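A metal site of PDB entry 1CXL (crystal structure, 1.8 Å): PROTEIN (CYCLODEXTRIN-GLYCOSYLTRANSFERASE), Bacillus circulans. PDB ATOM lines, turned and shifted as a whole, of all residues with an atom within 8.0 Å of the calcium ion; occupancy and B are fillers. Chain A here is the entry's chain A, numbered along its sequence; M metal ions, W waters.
The calcium ion is bound by water W3 (2.3 Å), water W2 (2.4 Å), OD1 of Asn 139 (2.4 Å), O of His 233 (2.4 Å), water W1 (2.4 Å), OD2 of Asp 199 (2.5 Å), O of Ile 190 (2.5 Å) and OD1 of Asp 199 (2.5 Å). The calcium ion has eight donor atoms within binding distance.
Water W1 bridges O of Asn 139 (2.7 Å) and O of Leu 200 (2.8 Å).
The nearest printed residue that does not touch the calcium ion is Met 234 (4.5 Å).
N of His 176 is in hydrogen-bond range of O of Asp 199, at 2.7 Å. N of Asp 199 lies close to OD1 of Asn 193, 3.2 Å away. A ring nitrogen (ND1) of His 233 is in hydrogen-bond range of the backbone carbonyl oxygen of Gly 189 (2.8 Å). The side-chain sulfur (SD) of Met 234 sits close to the backbone NH (N) of Asn 139 (3.6 Å). ND2 of Asn 139 is in hydrogen-bond range of ND1 of His 140 (2.9 Å). N of Leu 200 lies within hydrogen-bond range of O of Asn 139, 3.1 Å away.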
ATOM      1  N   PRO A 138     -18.281  26.520  26.285  1.00  0.00           N
ATOM      2  CA  PRO A 138     -18.808  27.670  25.571  1.00  0.00           C
ATOM      3  C   PRO A 138     -19.398  27.336  24.220  1.00  0.00           C
ATOM      4  O   PRO A 138     -19.710  28.241  23.436  1.00  0.00           O
ATOM      5  CB  PRO A 138     -17.609  28.586  25.337  1.00  0.00           C
ATOM      6  CG  PRO A 138     -16.376  27.696  25.408  1.00  0.00           C
ATOM      7  CD  PRO A 138     -16.796  26.465  26.213  1.00  0.00           C
ATOM      8  N   ASN A 139     -19.527  26.064  23.915  1.00  0.00           N
ATOM      9  CA  ASN A 139     -20.087  25.713  22.633  1.00  0.00           C
ATOM     10  C   ASN A 139     -21.588  25.891  22.601  1.00  0.00           C
ATOM     11  O   ASN A 139     -22.179  26.122  21.551  1.00  0.00           O
ATOM     12  CB  ASN A 139     -19.816  24.249  22.243  1.00  0.00           C
ATOM     13  CG  ASN A 139     -20.575  23.865  20.994  1.00  0.00           C
ATOM     14  OD1 ASN A 139     -20.268  24.347  19.890  1.00  0.00           O
ATOM     15  ND2 ASN A 139     -21.590  23.023  21.156  1.00  0.00           N
ATOM     16  N   HIS A 140     -22.225  25.712  23.764  1.00  0.00           N
ATOM     17  CA  HIS A 140     -23.679  25.763  23.818  1.00  0.00           C
ATOM     18  C   HIS A 140     -24.213  26.088  25.197  1.00  0.00           C
ATOM     19  O   HIS A 140     -23.481  26.167  26.174  1.00  0.00           O
ATOM     20  CB  HIS A 140     -24.192  24.332  23.493  1.00  0.00           C
ATOM     21  CG  HIS A 140     -23.506  23.309  24.359  1.00  0.00           C
ATOM     22  ND1 HIS A 140     -22.366  22.621  23.920  1.00  0.00           N
ATOM     23  CD2 HIS A 140     -23.782  22.888  25.626  1.00  0.00           C
ATOM     24  CE1 HIS A 140     -21.998  21.808  24.903  1.00  0.00           C
ATOM     25  NE2 HIS A 140     -22.818  21.947  25.952  1.00  0.00           N
ATOM     26  N   HIS A 176     -27.072  29.410  16.615  1.00  0.00           N
ATOM     27  CA  HIS A 176     -27.095  28.908  15.251  1.00  0.00           C
ATOM     28  C   HIS A 176     -28.420  28.227  15.017  1.00  0.00           C
ATOM     29  O   HIS A 176     -28.923  27.543  15.902  1.00  0.00           O
ATOM     30  CB  HIS A 176     -25.966  27.911  14.952  1.00  0.00           C
ATOM     31  CG  HIS A 176     -24.628  28.560  14.833  1.00  0.00           C
ATOM     32  ND1 HIS A 176     -23.532  28.072  15.523  1.00  0.00           N
ATOM     33  CD2 HIS A 176     -24.236  29.639  14.109  1.00  0.00           C
ATOM     34  CE1 HIS A 176     -22.505  28.862  15.208  1.00  0.00           C
ATOM     35  NE2 HIS A 176     -22.890  29.814  14.367  1.00  0.00           N
ATOM     36  N   GLU A 187     -17.012  20.880   9.531  1.00  0.00           N
ATOM     37  CA  GLU A 187     -17.867  22.053   9.359  1.00  0.00           C
ATOM     38  C   GLU A 187     -19.296  21.773   9.839  1.00  0.00           C
ATOM     39  O   GLU A 187     -19.919  22.600  10.509  1.00  0.00           O
ATOM     40  CB  GLU A 187     -17.854  22.501   7.893  1.00  0.00           C
ATOM     41  CG  GLU A 187     -18.945  23.516   7.540  1.00  0.00           C
ATOM     42  CD  GLU A 187     -18.977  23.759   6.065  1.00  0.00           C
ATOM     43  OE1 GLU A 187     -18.373  23.081   5.268  1.00  0.00           O
ATOM     44  OE2 GLU A 187     -19.671  24.804   5.745  1.00  0.00           O
ATOM     45  N   ASN A 188     -19.797  20.603   9.485  1.00  0.00           N
ATOM     46  CA  ASN A 188     -21.132  20.192   9.883  1.00  0.00           C
ATOM     47  C   ASN A 188     -21.277  20.200  11.402  1.00  0.00           C
ATOM     48  O   ASN A 188     -22.268  20.679  11.974  1.00  0.00           O
ATOM     49  CB  ASN A 188     -21.450  18.794   9.322  1.00  0.00           C
ATOM     50  CG  ASN A 188     -22.908  18.407   9.469  1.00  0.00           C
ATOM     51  OD1 ASN A 188     -23.385  18.109  10.562  1.00  0.00           O
ATOM     52  ND2 ASN A 188     -23.630  18.430   8.345  1.00  0.00           N
ATOM     53  N   GLY A 189     -20.264  19.672  12.071  1.00  0.00           N
ATOM     54  CA  GLY A 189     -20.248  19.584  13.509  1.00  0.00           C
ATOM     55  C   GLY A 189     -20.035  20.910  14.217  1.00  0.00           C
ATOM     56  O   GLY A 189     -20.327  21.043  15.408  1.00  0.00           O
ATOM     57  N   ILE A 190     -19.530  21.898  13.513  1.00  0.00           N
ATOM     58  CA  ILE A 190     -19.279  23.199  14.126  1.00  0.00           C
ATOM     59  C   ILE A 190     -20.497  24.106  14.130  1.00  0.00           C
ATOM     60  O   ILE A 190     -20.840  24.680  15.156  1.00  0.00           O
ATOM     61  CB  ILE A 190     -18.098  23.906  13.449  1.00  0.00           C
ATOM     62  CG1 ILE A 190     -16.780  23.248  13.840  1.00  0.00           C
ATOM     63  CG2 ILE A 190     -18.080  25.392  13.806  1.00  0.00           C
ATOM     64  CD1 ILE A 190     -15.580  23.745  13.019  1.00  0.00           C
ATOM     65  N   TYR A 191     -21.119  24.228  12.959  1.00  0.00           N
ATOM     66  CA  TYR A 191     -22.251  25.133  12.715  1.00  0.00           C
ATOM     67  C   TYR A 191     -23.672  24.621  12.944  1.00  0.00           C
ATOM     68  O   TYR A 191     -24.637  25.377  12.812  1.00  0.00           O
ATOM     69  CB  TYR A 191     -22.062  25.922  11.407  1.00  0.00           C
ATOM     70  CG  TYR A 191     -20.749  26.692  11.415  1.00  0.00           C
ATOM     71  CD1 TYR A 191     -20.637  27.900  12.089  1.00  0.00           C
ATOM     72  CD2 TYR A 191     -19.619  26.181  10.776  1.00  0.00           C
ATOM     73  CE1 TYR A 191     -19.442  28.611  12.114  1.00  0.00           C
ATOM     74  CE2 TYR A 191     -18.407  26.868  10.797  1.00  0.00           C
ATOM     75  CZ  TYR A 191     -18.318  28.094  11.461  1.00  0.00           C
ATOM     76  OH  TYR A 191     -17.139  28.779  11.476  1.00  0.00           O
ATOM     77  N   LYS A 192     -23.801  23.352  13.300  1.00  0.00           N
ATOM     78  CA  LYS A 192     -25.088  22.757  13.604  1.00  0.00           C
ATOM     79  C   LYS A 192     -25.095  22.378  15.075  1.00  0.00           C
ATOM     80  O   LYS A 192     -24.039  22.313  15.705  1.00  0.00           O
ATOM     81  CB  LYS A 192     -25.411  21.566  12.711  1.00  0.00           C
ATOM     82  CG  LYS A 192     -25.328  21.937  11.244  1.00  0.00           C
ATOM     83  CD  LYS A 192     -25.965  20.929  10.302  1.00  0.00           C
ATOM     84  CE  LYS A 192     -25.615  21.238   8.843  1.00  0.00           C
ATOM     85  NZ  LYS A 192     -26.386  20.453   7.864  1.00  0.00           N
ATOM     86  N   ASN A 193     -26.278  22.144  15.647  1.00  0.00           N
ATOM     87  CA  ASN A 193     -26.382  21.807  17.060  1.00  0.00           C
ATOM     88  C   ASN A 193     -25.896  20.402  17.396  1.00  0.00           C
ATOM     89  O   ASN A 193     -26.101  19.466  16.630  1.00  0.00           O
ATOM     90  CB  ASN A 193     -27.844  21.886  17.548  1.00  0.00           C
ATOM     91  CG  ASN A 193     -28.468  23.237  17.365  1.00  0.00           C
ATOM     92  OD1 ASN A 193     -27.787  24.275  17.367  1.00  0.00           O
ATOM     93  ND2 ASN A 193     -29.797  23.246  17.234  1.00  0.00           N
ATOM     94  N   LEU A 194     -25.296  20.262  18.578  1.00  0.00           N
ATOM     95  CA  LEU A 194     -24.882  18.973  19.084  1.00  0.00           C
ATOM     96  C   LEU A 194     -26.136  18.435  19.709  1.00  0.00           C
ATOM     97  O   LEU A 194     -26.593  18.954  20.720  1.00  0.00           O
ATOM     98  CB  LEU A 194     -23.860  19.106  20.231  1.00  0.00           C
ATOM     99  CG  LEU A 194     -22.417  19.240  19.798  1.00  0.00           C
ATOM    100  CD1 LEU A 194     -21.560  19.406  21.042  1.00  0.00           C
ATOM    101  CD2 LEU A 194     -21.996  17.985  19.042  1.00  0.00           C
ATOM    102  N   LEU A 197     -28.755  20.654  21.814  1.00  0.00           N
ATOM    103  CA  LEU A 197     -28.125  21.736  22.555  1.00  0.00           C
ATOM    104  C   LEU A 197     -28.073  23.017  21.756  1.00  0.00           C
ATOM    105  O   LEU A 197     -27.544  23.036  20.645  1.00  0.00           O
ATOM    106  CB  LEU A 197     -26.710  21.360  23.062  1.00  0.00           C
ATOM    107  CG  LEU A 197     -26.657  20.069  23.901  1.00  0.00           C
ATOM    108  CD1 LEU A 197     -25.198  19.631  24.070  1.00  0.00           C
ATOM    109  CD2 LEU A 197     -27.296  20.295  25.269  1.00  0.00           C
ATOM    110  N   ALA A 198     -28.636  24.086  22.310  1.00  0.00           N
ATOM    111  CA  ALA A 198     -28.632  25.373  21.611  1.00  0.00           C
ATOM    112  C   ALA A 198     -27.202  25.810  21.317  1.00  0.00           C
ATOM    113  O   ALA A 198     -26.438  26.120  22.229  1.00  0.00           O
ATOM    114  CB  ALA A 198     -29.364  26.420  22.425  1.00  0.00           C
ATOM    115  N   ASP A 199     -26.841  25.831  20.032  1.00  0.00           N
ATOM    116  CA  ASP A 199     -25.502  26.196  19.600  1.00  0.00           C
ATOM    117  C   ASP A 199     -25.240  27.678  19.621  1.00  0.00           C
ATOM    118  O   ASP A 199     -25.843  28.430  18.843  1.00  0.00           O
ATOM    119  CB  ASP A 199     -25.184  25.644  18.193  1.00  0.00           C
ATOM    120  CG  ASP A 199     -23.738  25.261  18.022  1.00  0.00           C
ATOM    121  OD1 ASP A 199     -23.154  24.504  18.790  1.00  0.00           O
ATOM    122  OD2 ASP A 199     -23.171  25.811  16.972  1.00  0.00           O
ATOM    123  N   LEU A 200     -24.324  28.097  20.480  1.00  0.00           N
ATOM    124  CA  LEU A 200     -23.980  29.508  20.573  1.00  0.00           C
ATOM    125  C   LEU A 200     -23.302  29.984  19.298  1.00  0.00           C
ATOM    126  O   LEU A 200     -22.496  29.271  18.701  1.00  0.00           O
ATOM    127  CB  LEU A 200     -23.092  29.815  21.794  1.00  0.00           C
ATOM    128  CG  LEU A 200     -23.842  29.730  23.127  1.00  0.00           C
ATOM    129  CD1 LEU A 200     -22.836  29.627  24.280  1.00  0.00           C
ATOM    130  CD2 LEU A 200     -24.722  30.969  23.303  1.00  0.00           C
ATOM    131  N   ASN A 201     -23.660  31.208  18.873  1.00  0.00           N
ATOM    132  CA  ASN A 201     -23.098  31.812  17.678  1.00  0.00           C
ATOM    133  C   ASN A 201     -21.913  32.679  18.051  1.00  0.00           C
ATOM    134  O   ASN A 201     -22.091  33.816  18.476  1.00  0.00           O
ATOM    135  CB  ASN A 201     -24.164  32.644  16.928  1.00  0.00           C
ATOM    136  CG  ASN A 201     -23.621  33.292  15.680  1.00  0.00           C
ATOM    137  OD1 ASN A 201     -22.500  33.011  15.248  1.00  0.00           O
ATOM    138  ND2 ASN A 201     -24.403  34.209  15.109  1.00  0.00           N
ATOM    139  N   HIS A 202     -20.709  32.131  17.897  1.00  0.00           N
ATOM    140  CA  HIS A 202     -19.486  32.858  18.250  1.00  0.00           C
ATOM    141  C   HIS A 202     -19.167  34.015  17.323  1.00  0.00           C
ATOM    142  O   HIS A 202     -18.239  34.787  17.552  1.00  0.00           O
ATOM    143  CB  HIS A 202     -18.291  31.891  18.467  1.00  0.00           C
ATOM    144  CG  HIS A 202     -18.590  30.931  19.567  1.00  0.00           C
ATOM    145  ND1 HIS A 202     -19.204  29.718  19.323  1.00  0.00           N
ATOM    146  CD2 HIS A 202     -18.400  31.036  20.911  1.00  0.00           C
ATOM    147  CE1 HIS A 202     -19.371  29.121  20.493  1.00  0.00           C
ATOM    148  NE2 HIS A 202     -18.895  29.881  21.468  1.00  0.00           N
ATOM    149  N   ALA A 230     -15.925  20.209  23.877  1.00  0.00           N
ATOM    150  CA  ALA A 230     -16.295  20.210  22.448  1.00  0.00           C
ATOM    151  C   ALA A 230     -15.536  21.162  21.534  1.00  0.00           C
ATOM    152  O   ALA A 230     -16.158  21.888  20.755  1.00  0.00           O
ATOM    153  CB  ALA A 230     -17.782  20.497  22.360  1.00  0.00           C
ATOM    154  N   LYS A 232     -13.930  20.545  18.924  1.00  0.00           N
ATOM    155  CA  LYS A 232     -14.067  20.231  17.510  1.00  0.00           C
ATOM    156  C   LYS A 232     -15.370  20.825  16.977  1.00  0.00           C
ATOM    157  O   LYS A 232     -15.623  20.816  15.774  1.00  0.00           O
ATOM    158  CB  LYS A 232     -14.104  18.731  17.276  1.00  0.00           C
ATOM    159  CG  LYS A 232     -13.887  18.366  15.814  1.00  0.00           C
ATOM    160  CD  LYS A 232     -13.977  16.871  15.554  1.00  0.00           C
ATOM    161  CE  LYS A 232     -13.719  16.506  14.101  1.00  0.00           C
ATOM    162  NZ  LYS A 232     -13.943  15.075  13.821  1.00  0.00           N
ATOM    163  N   HIS A 233     -16.190  21.345  17.906  1.00  0.00           N
ATOM    164  CA  HIS A 233     -17.509  21.888  17.588  1.00  0.00           C
ATOM    165  C   HIS A 233     -17.659  23.396  17.571  1.00  0.00           C
ATOM    166  O   HIS A 233     -18.758  23.906  17.418  1.00  0.00           O
ATOM    167  CB  HIS A 233     -18.594  21.187  18.426  1.00  0.00           C
ATOM    168  CG  HIS A 233     -18.563  19.700  18.205  1.00  0.00           C
ATOM    169  ND1 HIS A 233     -19.124  19.129  17.071  1.00  0.00           N
ATOM    170  CD2 HIS A 233     -18.006  18.704  18.951  1.00  0.00           C
ATOM    171  CE1 HIS A 233     -18.918  17.824  17.169  1.00  0.00           C
ATOM    172  NE2 HIS A 233     -18.256  17.537  18.276  1.00  0.00           N
ATOM    173  N   MET A 234     -16.548  24.111  17.699  1.00  0.00           N
ATOM    174  CA  MET A 234     -16.508  25.569  17.663  1.00  0.00           C
ATOM    175  C   MET A 234     -15.493  26.016  16.624  1.00  0.00           C
ATOM    176  O   MET A 234     -14.510  25.304  16.374  1.00  0.00           O
ATOM    177  CB  MET A 234     -16.156  26.169  19.051  1.00  0.00           C
ATOM    178  CG  MET A 234     -17.213  25.906  20.100  1.00  0.00           C
ATOM    179  SD  MET A 234     -16.731  26.491  21.732  1.00  0.00           S
ATOM    180  CE  MET A 234     -15.606  25.145  22.235  1.00  0.00           C
ATOM    181  N   PRO A 235     -15.706  27.184  16.012  1.00  0.00           N
ATOM    182  CA  PRO A 235     -14.774  27.644  15.009  1.00  0.00           C
ATOM    183  C   PRO A 235     -13.377  27.739  15.582  1.00  0.00           C
ATOM    184  O   PRO A 235     -13.153  28.326  16.636  1.00  0.00           O
ATOM    185  CB  PRO A 235     -15.280  29.032  14.540  1.00  0.00           C
ATOM    186  CG  PRO A 235     -16.701  29.150  15.061  1.00  0.00           C
ATOM    187  CD  PRO A 235     -16.853  28.132  16.177  1.00  0.00           C
HETATM  188 CA    CA M   1     -20.942  24.902  17.657  1.00  0.00          CA
HETATM  189  O   HOH W   1     -21.174  26.800  19.148  1.00  0.00           O
HETATM  190  O   HOH W   2     -21.630  22.700  17.146  1.00  0.00           O
HETATM  191  O   HOH W   3     -19.887  26.718  16.623  1.00  0.00           O
